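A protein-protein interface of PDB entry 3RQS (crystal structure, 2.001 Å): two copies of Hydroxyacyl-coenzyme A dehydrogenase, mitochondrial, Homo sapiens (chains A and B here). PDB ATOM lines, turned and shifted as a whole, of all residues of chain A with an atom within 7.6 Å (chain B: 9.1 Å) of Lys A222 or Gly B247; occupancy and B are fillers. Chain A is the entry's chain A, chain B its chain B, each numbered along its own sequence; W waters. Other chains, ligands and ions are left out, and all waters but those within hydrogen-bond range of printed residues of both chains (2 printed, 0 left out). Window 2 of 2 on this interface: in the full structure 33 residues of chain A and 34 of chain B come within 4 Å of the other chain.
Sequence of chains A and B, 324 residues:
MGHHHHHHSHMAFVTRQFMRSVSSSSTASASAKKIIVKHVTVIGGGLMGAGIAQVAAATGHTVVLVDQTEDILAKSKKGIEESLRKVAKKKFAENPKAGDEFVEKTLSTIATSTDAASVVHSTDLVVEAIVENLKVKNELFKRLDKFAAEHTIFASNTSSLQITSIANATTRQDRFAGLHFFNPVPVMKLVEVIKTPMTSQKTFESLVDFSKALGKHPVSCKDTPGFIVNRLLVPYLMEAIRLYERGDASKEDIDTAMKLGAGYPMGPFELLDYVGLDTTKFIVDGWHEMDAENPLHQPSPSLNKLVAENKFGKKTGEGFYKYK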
ATOM      1  N   GLN A 162     -14.830  15.804  20.179  1.00  0.00           N
ATOM      2  CA  GLN A 162     -14.532  14.937  19.062  1.00  0.00           C
ATOM      3  C   GLN A 162     -15.845  14.513  18.424  1.00  0.00           C
ATOM      4  O   GLN A 162     -16.803  14.159  19.109  1.00  0.00           O
ATOM      5  CB  GLN A 162     -13.711  13.724  19.499  1.00  0.00           C
ATOM      6  CG  GLN A 162     -12.221  14.002  19.551  1.00  0.00           C
ATOM      7  CD  GLN A 162     -11.392  12.735  19.507  1.00  0.00           C
ATOM      8  OE1 GLN A 162     -11.867  11.657  19.866  1.00  0.00           O
ATOM      9  NE2 GLN A 162     -10.146  12.857  19.057  1.00  0.00           N
ATOM     10  N   ILE A 163     -15.893  14.576  17.104  1.00  0.00           N
ATOM     11  CA  ILE A 163     -17.086  14.178  16.392  1.00  0.00           C
ATOM     12  C   ILE A 163     -17.418  12.730  16.729  1.00  0.00           C
ATOM     13  O   ILE A 163     -18.578  12.367  16.853  1.00  0.00           O
ATOM     14  CB  ILE A 163     -16.883  14.311  14.888  1.00  0.00           C
ATOM     15  CG1 ILE A 163     -16.440  15.743  14.548  1.00  0.00           C
ATOM     16  CG2 ILE A 163     -18.157  13.907  14.147  1.00  0.00           C
ATOM     17  CD1 ILE A 163     -17.423  16.803  15.004  1.00  0.00           C
ATOM     18  N   VAL A 193     -14.555  20.006   6.944  1.00  0.00           N
ATOM     19  CA  VAL A 193     -15.376  18.807   6.928  1.00  0.00           C
ATOM     20  C   VAL A 193     -14.603  17.691   7.627  1.00  0.00           C
ATOM     21  O   VAL A 193     -13.500  17.335   7.215  1.00  0.00           O
ATOM     22  CB  VAL A 193     -15.733  18.398   5.500  1.00  0.00           C
ATOM     23  CG1 VAL A 193     -16.736  17.278   5.533  1.00  0.00           C
ATOM     24  CG2 VAL A 193     -16.301  19.612   4.713  1.00  0.00           C
ATOM     25  N   ILE A 194     -15.176  17.151   8.695  1.00  0.00           N
ATOM     26  CA  ILE A 194     -14.454  16.189   9.524  1.00  0.00           C
ATOM     27  C   ILE A 194     -15.062  14.797   9.424  1.00  0.00           C
ATOM     28  O   ILE A 194     -16.205  14.589   9.831  1.00  0.00           O
ATOM     29  CB  ILE A 194     -14.469  16.615  11.002  1.00  0.00           C
ATOM     30  CG1 ILE A 194     -14.060  18.081  11.149  1.00  0.00           C
ATOM     31  CG2 ILE A 194     -13.562  15.707  11.829  1.00  0.00           C
ATOM     32  CD1 ILE A 194     -12.710  18.408  10.517  1.00  0.00           C
ATOM     33  N   LYS A 195     -14.306  13.847   8.876  1.00  0.00           N
ATOM     34  CA  LYS A 195     -14.708  12.445   8.921  1.00  0.00           C
ATOM     35  C   LYS A 195     -14.178  11.826  10.206  1.00  0.00           C
ATOM     36  O   LYS A 195     -13.057  12.116  10.625  1.00  0.00           O
ATOM     37  CB  LYS A 195     -14.131  11.659   7.738  1.00  0.00           C
ATOM     38  CG  LYS A 195     -14.721  11.992   6.388  1.00  0.00           C
ATOM     39  CD  LYS A 195     -14.020  11.215   5.274  1.00  0.00           C
ATOM     40  CE  LYS A 195     -14.478   9.762   5.225  1.00  0.00           C
ATOM     41  NZ  LYS A 195     -13.781   8.975   4.158  1.00  0.00           N
ATOM     42  N   THR A 196     -14.984  10.977  10.831  1.00  0.00           N
ATOM     43  CA  THR A 196     -14.464  10.058  11.834  1.00  0.00           C
ATOM     44  C   THR A 196     -14.048   8.820  11.048  1.00  0.00           C
ATOM     45  O   THR A 196     -14.281   8.750   9.842  1.00  0.00           O
ATOM     46  CB  THR A 196     -15.539   9.680  12.860  1.00  0.00           C
ATOM     47  OG1 THR A 196     -16.438   8.742  12.273  1.00  0.00           O
ATOM     48  CG2 THR A 196     -16.316  10.916  13.299  1.00  0.00           C
ATOM     49  N   PRO A 197     -13.432   7.830  11.712  1.00  0.00           N
ATOM     50  CA  PRO A 197     -13.094   6.621  10.949  1.00  0.00           C
ATOM     51  C   PRO A 197     -14.335   5.875  10.443  1.00  0.00           C
ATOM     52  O   PRO A 197     -14.222   4.981   9.597  1.00  0.00           O
ATOM     53  CB  PRO A 197     -12.327   5.764  11.970  1.00  0.00           C
ATOM     54  CG  PRO A 197     -11.815   6.751  12.982  1.00  0.00           C
ATOM     55  CD  PRO A 197     -12.888   7.799  13.079  1.00  0.00           C
ATOM     56  N   SER A 220     -10.546  19.192   4.471  1.00  0.00           N
ATOM     57  CA  SER A 220     -10.717  17.945   5.179  1.00  0.00           C
ATOM     58  C   SER A 220      -9.739  17.860   6.354  1.00  0.00           C
ATOM     59  O   SER A 220      -8.578  18.246   6.240  1.00  0.00           O
ATOM     60  CB  SER A 220     -10.494  16.782   4.207  1.00  0.00           C
ATOM     61  OG  SER A 220     -10.586  15.543   4.880  1.00  0.00           O
ATOM     62  N   CYS A 221     -10.209  17.370   7.493  1.00  0.00           N
ATOM     63  CA  CYS A 221      -9.300  17.084   8.598  1.00  0.00           C
ATOM     64  C   CYS A 221      -9.786  15.849   9.324  1.00  0.00           C
ATOM     65  O   CYS A 221     -10.990  15.608   9.402  1.00  0.00           O
ATOM     66  CB  CYS A 221      -9.221  18.260   9.585  1.00  0.00           C
ATOM     67  SG  CYS A 221      -7.932  18.047  10.897  1.00  0.00           S
ATOM     68  N   LYS A 222      -8.855  15.075   9.864  1.00  0.00           N
ATOM     69  CA  LYS A 222      -9.230  13.989  10.754  1.00  0.00           C
ATOM     70  C   LYS A 222      -9.916  14.537  12.000  1.00  0.00           C
ATOM     71  O   LYS A 222      -9.775  15.719  12.330  1.00  0.00           O
ATOM     72  CB  LYS A 222      -8.009  13.153  11.138  1.00  0.00           C
ATOM     73  CG  LYS A 222      -7.478  12.319   9.995  1.00  0.00           C
ATOM     74  CD  LYS A 222      -6.640  11.153  10.496  1.00  0.00           C
ATOM     75  CE  LYS A 222      -5.900  10.488   9.350  1.00  0.00           C
ATOM     76  NZ  LYS A 222      -6.719  10.514   8.110  1.00  0.00           N
ATOM     77  N   ASP A 223     -10.656  13.673  12.690  1.00  0.00           N
ATOM     78  CA  ASP A 223     -11.366  14.056  13.904  1.00  0.00           C
ATOM     79  C   ASP A 223     -10.408  14.213  15.095  1.00  0.00           C
ATOM     80  O   ASP A 223     -10.427  13.434  16.050  1.00  0.00           O
ATOM     81  CB  ASP A 223     -12.461  13.031  14.217  1.00  0.00           C
ATOM     82  CG  ASP A 223     -13.249  13.392  15.447  1.00  0.00           C
ATOM     83  OD1 ASP A 223     -13.275  14.590  15.787  1.00  0.00           O
ATOM     84  OD2 ASP A 223     -13.836  12.487  16.083  1.00  0.00           O
ATOM     85  N   THR A 224      -9.576  15.239  15.024  1.00  0.00           N
ATOM     86  CA  THR A 224      -8.550  15.497  16.022  1.00  0.00           C
ATOM     87  C   THR A 224      -8.833  16.849  16.664  1.00  0.00           C
ATOM     88  O   THR A 224      -9.440  17.718  16.040  1.00  0.00           O
ATOM     89  CB  THR A 224      -7.157  15.497  15.361  1.00  0.00           C
ATOM     90  OG1 THR A 224      -7.170  16.394  14.241  1.00  0.00           O
ATOM     91  CG2 THR A 224      -6.815  14.096  14.856  1.00  0.00           C
ATOM     92  N   PRO A 225      -8.407  17.031  17.923  1.00  0.00           N
ATOM     93  CA  PRO A 225      -8.754  18.248  18.666  1.00  0.00           C
ATOM     94  C   PRO A 225      -8.332  19.521  17.938  1.00  0.00           C
ATOM     95  O   PRO A 225      -7.155  19.697  17.627  1.00  0.00           O
ATOM     96  CB  PRO A 225      -7.949  18.106  19.963  1.00  0.00           C
ATOM     97  CG  PRO A 225      -7.781  16.633  20.133  1.00  0.00           C
ATOM     98  CD  PRO A 225      -7.601  16.100  18.733  1.00  0.00           C
ATOM     99  N   GLY A 226      -9.292  20.405  17.700  1.00  0.00           N
ATOM    100  CA  GLY A 226      -9.028  21.678  17.052  1.00  0.00           C
ATOM    101  C   GLY A 226      -9.020  21.598  15.536  1.00  0.00           C
ATOM    102  O   GLY A 226      -8.924  22.620  14.855  1.00  0.00           O
ATOM    103  N   PHE A 227      -9.130  20.385  15.006  1.00  0.00           N
ATOM    104  CA  PHE A 227      -9.119  20.195  13.562  1.00  0.00           C
ATOM    105  C   PHE A 227      -7.889  20.913  13.011  1.00  0.00           C
ATOM    106  O   PHE A 227      -6.795  20.709  13.515  1.00  0.00           O
ATOM    107  CB  PHE A 227     -10.404  20.749  12.950  1.00  0.00           C
ATOM    108  CG  PHE A 227     -11.663  20.175  13.558  1.00  0.00           C
ATOM    109  CD1 PHE A 227     -11.720  18.847  13.946  1.00  0.00           C
ATOM    110  CD2 PHE A 227     -12.787  20.970  13.744  1.00  0.00           C
ATOM    111  CE1 PHE A 227     -12.875  18.323  14.505  1.00  0.00           C
ATOM    112  CE2 PHE A 227     -13.945  20.447  14.302  1.00  0.00           C
ATOM    113  CZ  PHE A 227     -13.983  19.126  14.684  1.00  0.00           C
ATOM    114  N   ILE A 228      -8.057  21.766  12.002  1.00  0.00           N
ATOM    115  CA  ILE A 228      -6.910  22.535  11.515  1.00  0.00           C
ATOM    116  C   ILE A 228      -6.839  23.917  12.140  1.00  0.00           C
ATOM    117  O   ILE A 228      -5.881  24.247  12.837  1.00  0.00           O
ATOM    118  CB  ILE A 228      -6.914  22.718   9.990  1.00  0.00           C
ATOM    119  CG1 ILE A 228      -7.015  21.361   9.283  1.00  0.00           C
ATOM    120  CG2 ILE A 228      -5.638  23.449   9.555  1.00  0.00           C
ATOM    121  CD1 ILE A 228      -7.229  21.476   7.778  1.00  0.00           C
ATOM    122  N   ALA B 240       2.114  23.471  12.349  1.00  0.00           N
ATOM    123  CA  ALA B 240       1.470  23.168  11.081  1.00  0.00           C
ATOM    124  C   ALA B 240       2.167  21.980  10.437  1.00  0.00           C
ATOM    125  O   ALA B 240       1.517  21.065   9.936  1.00  0.00           O
ATOM    126  CB  ALA B 240       1.510  24.386  10.138  1.00  0.00           C
ATOM    127  N   ILE B 241       3.496  22.004  10.410  1.00  0.00           N
ATOM    128  CA  ILE B 241       4.217  20.867   9.845  1.00  0.00           C
ATOM    129  C   ILE B 241       3.816  19.602  10.593  1.00  0.00           C
ATOM    130  O   ILE B 241       3.543  18.580   9.977  1.00  0.00           O
ATOM    131  CB  ILE B 241       5.747  21.024   9.928  1.00  0.00           C
ATOM    132  CG1 ILE B 241       6.215  22.220   9.086  1.00  0.00           C
ATOM    133  CG2 ILE B 241       6.436  19.747   9.443  1.00  0.00           C
ATOM    134  CD1 ILE B 241       7.672  22.626   9.365  1.00  0.00           C
ATOM    135  N   ARG B 242       3.779  19.677  11.924  1.00  0.00           N
ATOM    136  CA  ARG B 242       3.499  18.482  12.729  1.00  0.00           C
ATOM    137  C   ARG B 242       2.106  17.918  12.461  1.00  0.00           C
ATOM    138  O   ARG B 242       1.917  16.706  12.429  1.00  0.00           O
ATOM    139  CB  ARG B 242       3.706  18.765  14.221  1.00  0.00           C
ATOM    140  CG  ARG B 242       5.159  19.057  14.568  1.00  0.00           C
ATOM    141  CD  ARG B 242       5.368  19.376  16.033  1.00  0.00           C
ATOM    142  NE  ARG B 242       6.724  19.865  16.250  1.00  0.00           N
ATOM    143  CZ  ARG B 242       7.017  21.032  16.815  1.00  0.00           C
ATOM    144  NH1 ARG B 242       6.045  21.820  17.234  1.00  0.00           N
ATOM    145  NH2 ARG B 242       8.283  21.404  16.962  1.00  0.00           N
ATOM    146  N   LEU B 243       1.134  18.801  12.255  1.00  0.00           N
ATOM    147  CA  LEU B 243      -0.221  18.370  11.972  1.00  0.00           C
ATOM    148  C   LEU B 243      -0.248  17.607  10.649  1.00  0.00           C
ATOM    149  O   LEU B 243      -0.864  16.544  10.527  1.00  0.00           O
ATOM    150  CB  LEU B 243      -1.157  19.582  11.934  1.00  0.00           C
ATOM    151  CG  LEU B 243      -2.667  19.346  11.885  1.00  0.00           C
ATOM    152  CD1 LEU B 243      -3.401  20.505  12.536  1.00  0.00           C
ATOM    153  CD2 LEU B 243      -3.126  19.180  10.460  1.00  0.00           C
ATOM    154  N   TYR B 244       0.451  18.150   9.660  1.00  0.00           N
ATOM    155  CA  TYR B 244       0.610  17.490   8.382  1.00  0.00           C
ATOM    156  C   TYR B 244       1.324  16.153   8.553  1.00  0.00           C
ATOM    157  O   TYR B 244       0.906  15.155   7.983  1.00  0.00           O
ATOM    158  CB  TYR B 244       1.408  18.389   7.442  1.00  0.00           C
ATOM    159  CG  TYR B 244       1.973  17.689   6.230  1.00  0.00           C
ATOM    160  CD1 TYR B 244       1.132  17.148   5.267  1.00  0.00           C
ATOM    161  CD2 TYR B 244       3.346  17.600   6.029  1.00  0.00           C
ATOM    162  CE1 TYR B 244       1.635  16.514   4.157  1.00  0.00           C
ATOM    163  CE2 TYR B 244       3.863  16.961   4.908  1.00  0.00           C
ATOM    164  CZ  TYR B 244       2.996  16.422   3.980  1.00  0.00           C
ATOM    165  OH  TYR B 244       3.488  15.792   2.856  1.00  0.00           O
ATOM    166  N   GLU B 245       2.407  16.136   9.331  1.00  0.00           N
ATOM    167  CA  GLU B 245       3.192  14.910   9.477  1.00  0.00           C
ATOM    168  C   GLU B 245       2.401  13.830  10.216  1.00  0.00           C
ATOM    169  O   GLU B 245       2.594  12.635   9.993  1.00  0.00           O
ATOM    170  CB  GLU B 245       4.522  15.187  10.176  1.00  0.00           C
ATOM    171  CG  GLU B 245       5.546  15.851   9.276  1.00  0.00           C
ATOM    172  CD  GLU B 245       6.869  16.096   9.969  1.00  0.00           C
ATOM    173  OE1 GLU B 245       6.872  16.661  11.083  1.00  0.00           O
ATOM    174  OE2 GLU B 245       7.910  15.707   9.401  1.00  0.00           O
ATOM    175  N   ARG B 246       1.503  14.254  11.096  1.00  0.00           N
ATOM    176  CA  ARG B 246       0.603  13.321  11.751  1.00  0.00           C
ATOM    177  C   ARG B 246      -0.345  12.674  10.748  1.00  0.00           C
ATOM    178  O   ARG B 246      -0.980  11.660  11.046  1.00  0.00           O
ATOM    179  CB  ARG B 246      -0.194  14.025  12.841  1.00  0.00           C
ATOM    180  CG  ARG B 246       0.570  14.149  14.123  1.00  0.00           C
ATOM    181  CD  ARG B 246      -0.372  14.448  15.273  1.00  0.00           C
ATOM    182  NE  ARG B 246      -1.066  15.718  15.099  1.00  0.00           N
ATOM    183  CZ  ARG B 246      -0.517  16.895  15.367  1.00  0.00           C
ATOM    184  NH1 ARG B 246       0.740  16.951  15.791  1.00  0.00           N
ATOM    185  NH2 ARG B 246      -1.220  18.012  15.207  1.00  0.00           N
ATOM    186  N   GLY B 247      -0.425  13.261   9.555  1.00  0.00           N
ATOM    187  CA  GLY B 247      -1.366  12.811   8.547  1.00  0.00           C
ATOM    188  C   GLY B 247      -2.788  13.313   8.761  1.00  0.00           C
ATOM    189  O   GLY B 247      -3.721  12.814   8.133  1.00  0.00           O
ATOM    190  N   ASP B 248      -2.962  14.297   9.643  1.00  0.00           N
ATOM    191  CA  ASP B 248      -4.302  14.768  10.009  1.00  0.00           C
ATOM    192  C   ASP B 248      -4.948  15.595   8.907  1.00  0.00           C
ATOM    193  O   ASP B 248      -6.181  15.695   8.820  1.00  0.00           O
ATOM    194  CB  ASP B 248      -4.253  15.607  11.284  1.00  0.00           C
ATOM    195  CG  ASP B 248      -3.850  14.797  12.493  1.00  0.00           C
ATOM    196  OD1 ASP B 248      -3.962  13.554  12.432  1.00  0.00           O
ATOM    197  OD2 ASP B 248      -3.427  15.404  13.492  1.00  0.00           O
ATOM    198  N   ALA B 249      -4.108  16.198   8.076  1.00  0.00           N
ATOM    199  CA  ALA B 249      -4.581  17.041   6.987  1.00  0.00           C
ATOM    200  C   ALA B 249      -3.447  17.315   6.008  1.00  0.00           C
ATOM    201  O   ALA B 249      -2.265  17.228   6.368  1.00  0.00           O
ATOM    202  CB  ALA B 249      -5.159  18.341   7.530  1.00  0.00           C
ATOM    203  N   SER B 250      -3.803  17.616   4.766  1.00  0.00           N
ATOM    204  CA  SER B 250      -2.799  17.865   3.748  1.00  0.00           C
ATOM    205  C   SER B 250      -2.220  19.277   3.894  1.00  0.00           C
ATOM    206  O   SER B 250      -2.839  20.145   4.503  1.00  0.00           O
ATOM    207  CB  SER B 250      -3.394  17.679   2.354  1.00  0.00           C
ATOM    208  OG  SER B 250      -4.317  18.710   2.069  1.00  0.00           O
ATOM    209  N   LYS B 251      -1.035  19.493   3.328  1.00  0.00           N
ATOM    210  CA  LYS B 251      -0.400  20.807   3.352  1.00  0.00           C
ATOM    211  C   LYS B 251      -1.326  21.817   2.691  1.00  0.00           C
ATOM    212  O   LYS B 251      -1.517  22.937   3.181  1.00  0.00           O
ATOM    213  CB  LYS B 251       0.940  20.768   2.599  1.00  0.00           C
ATOM    214  CG  LYS B 251       1.982  19.879   3.234  1.00  0.00           C
ATOM    215  CD  LYS B 251       3.330  20.056   2.546  1.00  0.00           C
ATOM    216  CE  LYS B 251       3.238  19.693   1.075  1.00  0.00           C
ATOM    217  NZ  LYS B 251       3.038  18.232   0.923  1.00  0.00           N
ATOM    218  N   ASP B 253      -4.609  21.780   2.224  1.00  0.00           N
ATOM    219  CA  ASP B 253      -5.767  22.101   3.059  1.00  0.00           C
ATOM    220  C   ASP B 253      -5.429  22.950   4.271  1.00  0.00           C
ATOM    221  O   ASP B 253      -6.215  23.808   4.667  1.00  0.00           O
ATOM    222  CB  ASP B 253      -6.493  20.832   3.499  1.00  0.00           C
ATOM    223  CG  ASP B 253      -7.453  20.332   2.444  1.00  0.00           C
ATOM    224  OD1 ASP B 253      -7.597  21.018   1.410  1.00  0.00           O
ATOM    225  OD2 ASP B 253      -8.070  19.271   2.649  1.00  0.00           O
ATOM    226  N   ILE B 254      -4.271  22.701   4.879  1.00  0.00           N
ATOM    227  CA  ILE B 254      -3.862  23.492   6.035  1.00  0.00           C
ATOM    228  C   ILE B 254      -3.615  24.930   5.585  1.00  0.00           C
ATOM    229  O   ILE B 254      -4.027  25.875   6.250  1.00  0.00           O
ATOM    230  CB  ILE B 254      -2.603  22.915   6.710  1.00  0.00           C
ATOM    231  CG1 ILE B 254      -2.901  21.524   7.287  1.00  0.00           C
ATOM    232  CG2 ILE B 254      -2.099  23.852   7.814  1.00  0.00           C
ATOM    233  CD1 ILE B 254      -1.647  20.736   7.686  1.00  0.00           C
ATOM    234  N   SER B 302      10.248  15.908   8.247  1.00  0.00           N
ATOM    235  CA  SER B 302       9.992  16.452   6.918  1.00  0.00           C
ATOM    236  C   SER B 302      10.856  17.672   6.669  1.00  0.00           C
ATOM    237  O   SER B 302      11.472  17.812   5.612  1.00  0.00           O
ATOM    238  CB  SER B 302       8.526  16.842   6.769  1.00  0.00           C
ATOM    239  OG  SER B 302       7.700  15.703   6.914  1.00  0.00           O
HETATM  240  O   HOH W   1      -3.997  17.341  15.041  1.00  0.00           O
HETATM  241  O   HOH W   2      -6.704  17.626   4.425  1.00  0.00           O
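The side-chain carboxylate of Asp B253 is in hydrogen-bond range of the backbone NH of Ser A220, 3.1 Å away.
SG of Cys A221 sits close to O of Asp B248 (3.6 Å).
The backbone carbonyl oxygen (O) of Asp B248 lies within hydrogen-bond range of the backbone NH (N) of Lys A222.
N of Cys A221 sits at hydrogen-bond distance from O of Val A193.
O of Lys A222 lies within hydrogen-bond range of OG1 of Thr A224.
The backbone NH (N) of Asp B248 is in hydrogen-bond range of the backbone carbonyl oxygen (O) of Leu B243 (3.2 Å).
The guanidinium group of Arg B246 is in salt-bridge range of the side-chain carboxylate of Asp B248 (2.9 Å).
OG of Ser B250 lies within hydrogen-bond range of N of Asp B253, 3.1 Å away.
Among the printed residues, merely in contact across the chains: Lys A222 with Gly B247 (3.4 Å), Phe A227 with Leu B243 (3.5 Å), Ser A220 with Ala B249 (3.7 Å), Ile A228 with Ala B249 (3.8 Å), Thr A224 with Asp B248 (3.8 Å) and Ile A228 with Ile B254 (3.9 Å).
Printed residues of chain B within 4 Å of Lys A222: Gly B247 (3.4 Å) and Asp B248 (2.9 Å).
Gly B247 touches one residue of chain A.
Of chain B, only Asp B248 (3.4 Å) comes within 4 Å of Cys A221.
Of the printed residues of chain B, Ile A228 touches Ala B249 and Ile B254.
Printed residues of chain A within 4 Å of Asp B253: Ser A220.
Printed residues of chain B within 4 Å of Ser A220: Ala B249 (3.7 Å) and Asp B253 (3.1 Å).
Of the printed residues of chain B, Phe A227 touches Leu B243.
Ile B241 touches none of the printed residues of chain A.
The nearest residue of chain B that does not touch Lys A222 is Ala B249 (5.2 Å).
The nearest residue of chain A that does not touch Gly B247 is Cys A221 (6.9 Å).
The nearest printed residue of chain B that does not touch Phe A227 is Asp B248 (6.1 Å).
Of the 16 printed residues of chain A, 6 touch a printed residue of chain B.
Hydrophobic or aromatic side chains of chain A that line the printed part of chain B: Ile A228.
Among the printed residues, no Asp or Glu carboxylate lies within 4 Å of a Lys or Arg side-chain nitrogen of the other chain.
No position is printed for both chains.
Of the 9 pairs that touch across the chains among the printed residues, none has its exchanged pair printed and touching as well.
Water W1 lies within hydrogen-bond range of OD2 of Asp B248, NH2 of Arg B246 and OG1 of Thr A224.
Water W2 lies within hydrogen-bond range of O of Ser A220 (2.7 Å), OD2 of Asp B253 (2.8 Å) and N of Ser B250 (2.9 Å).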
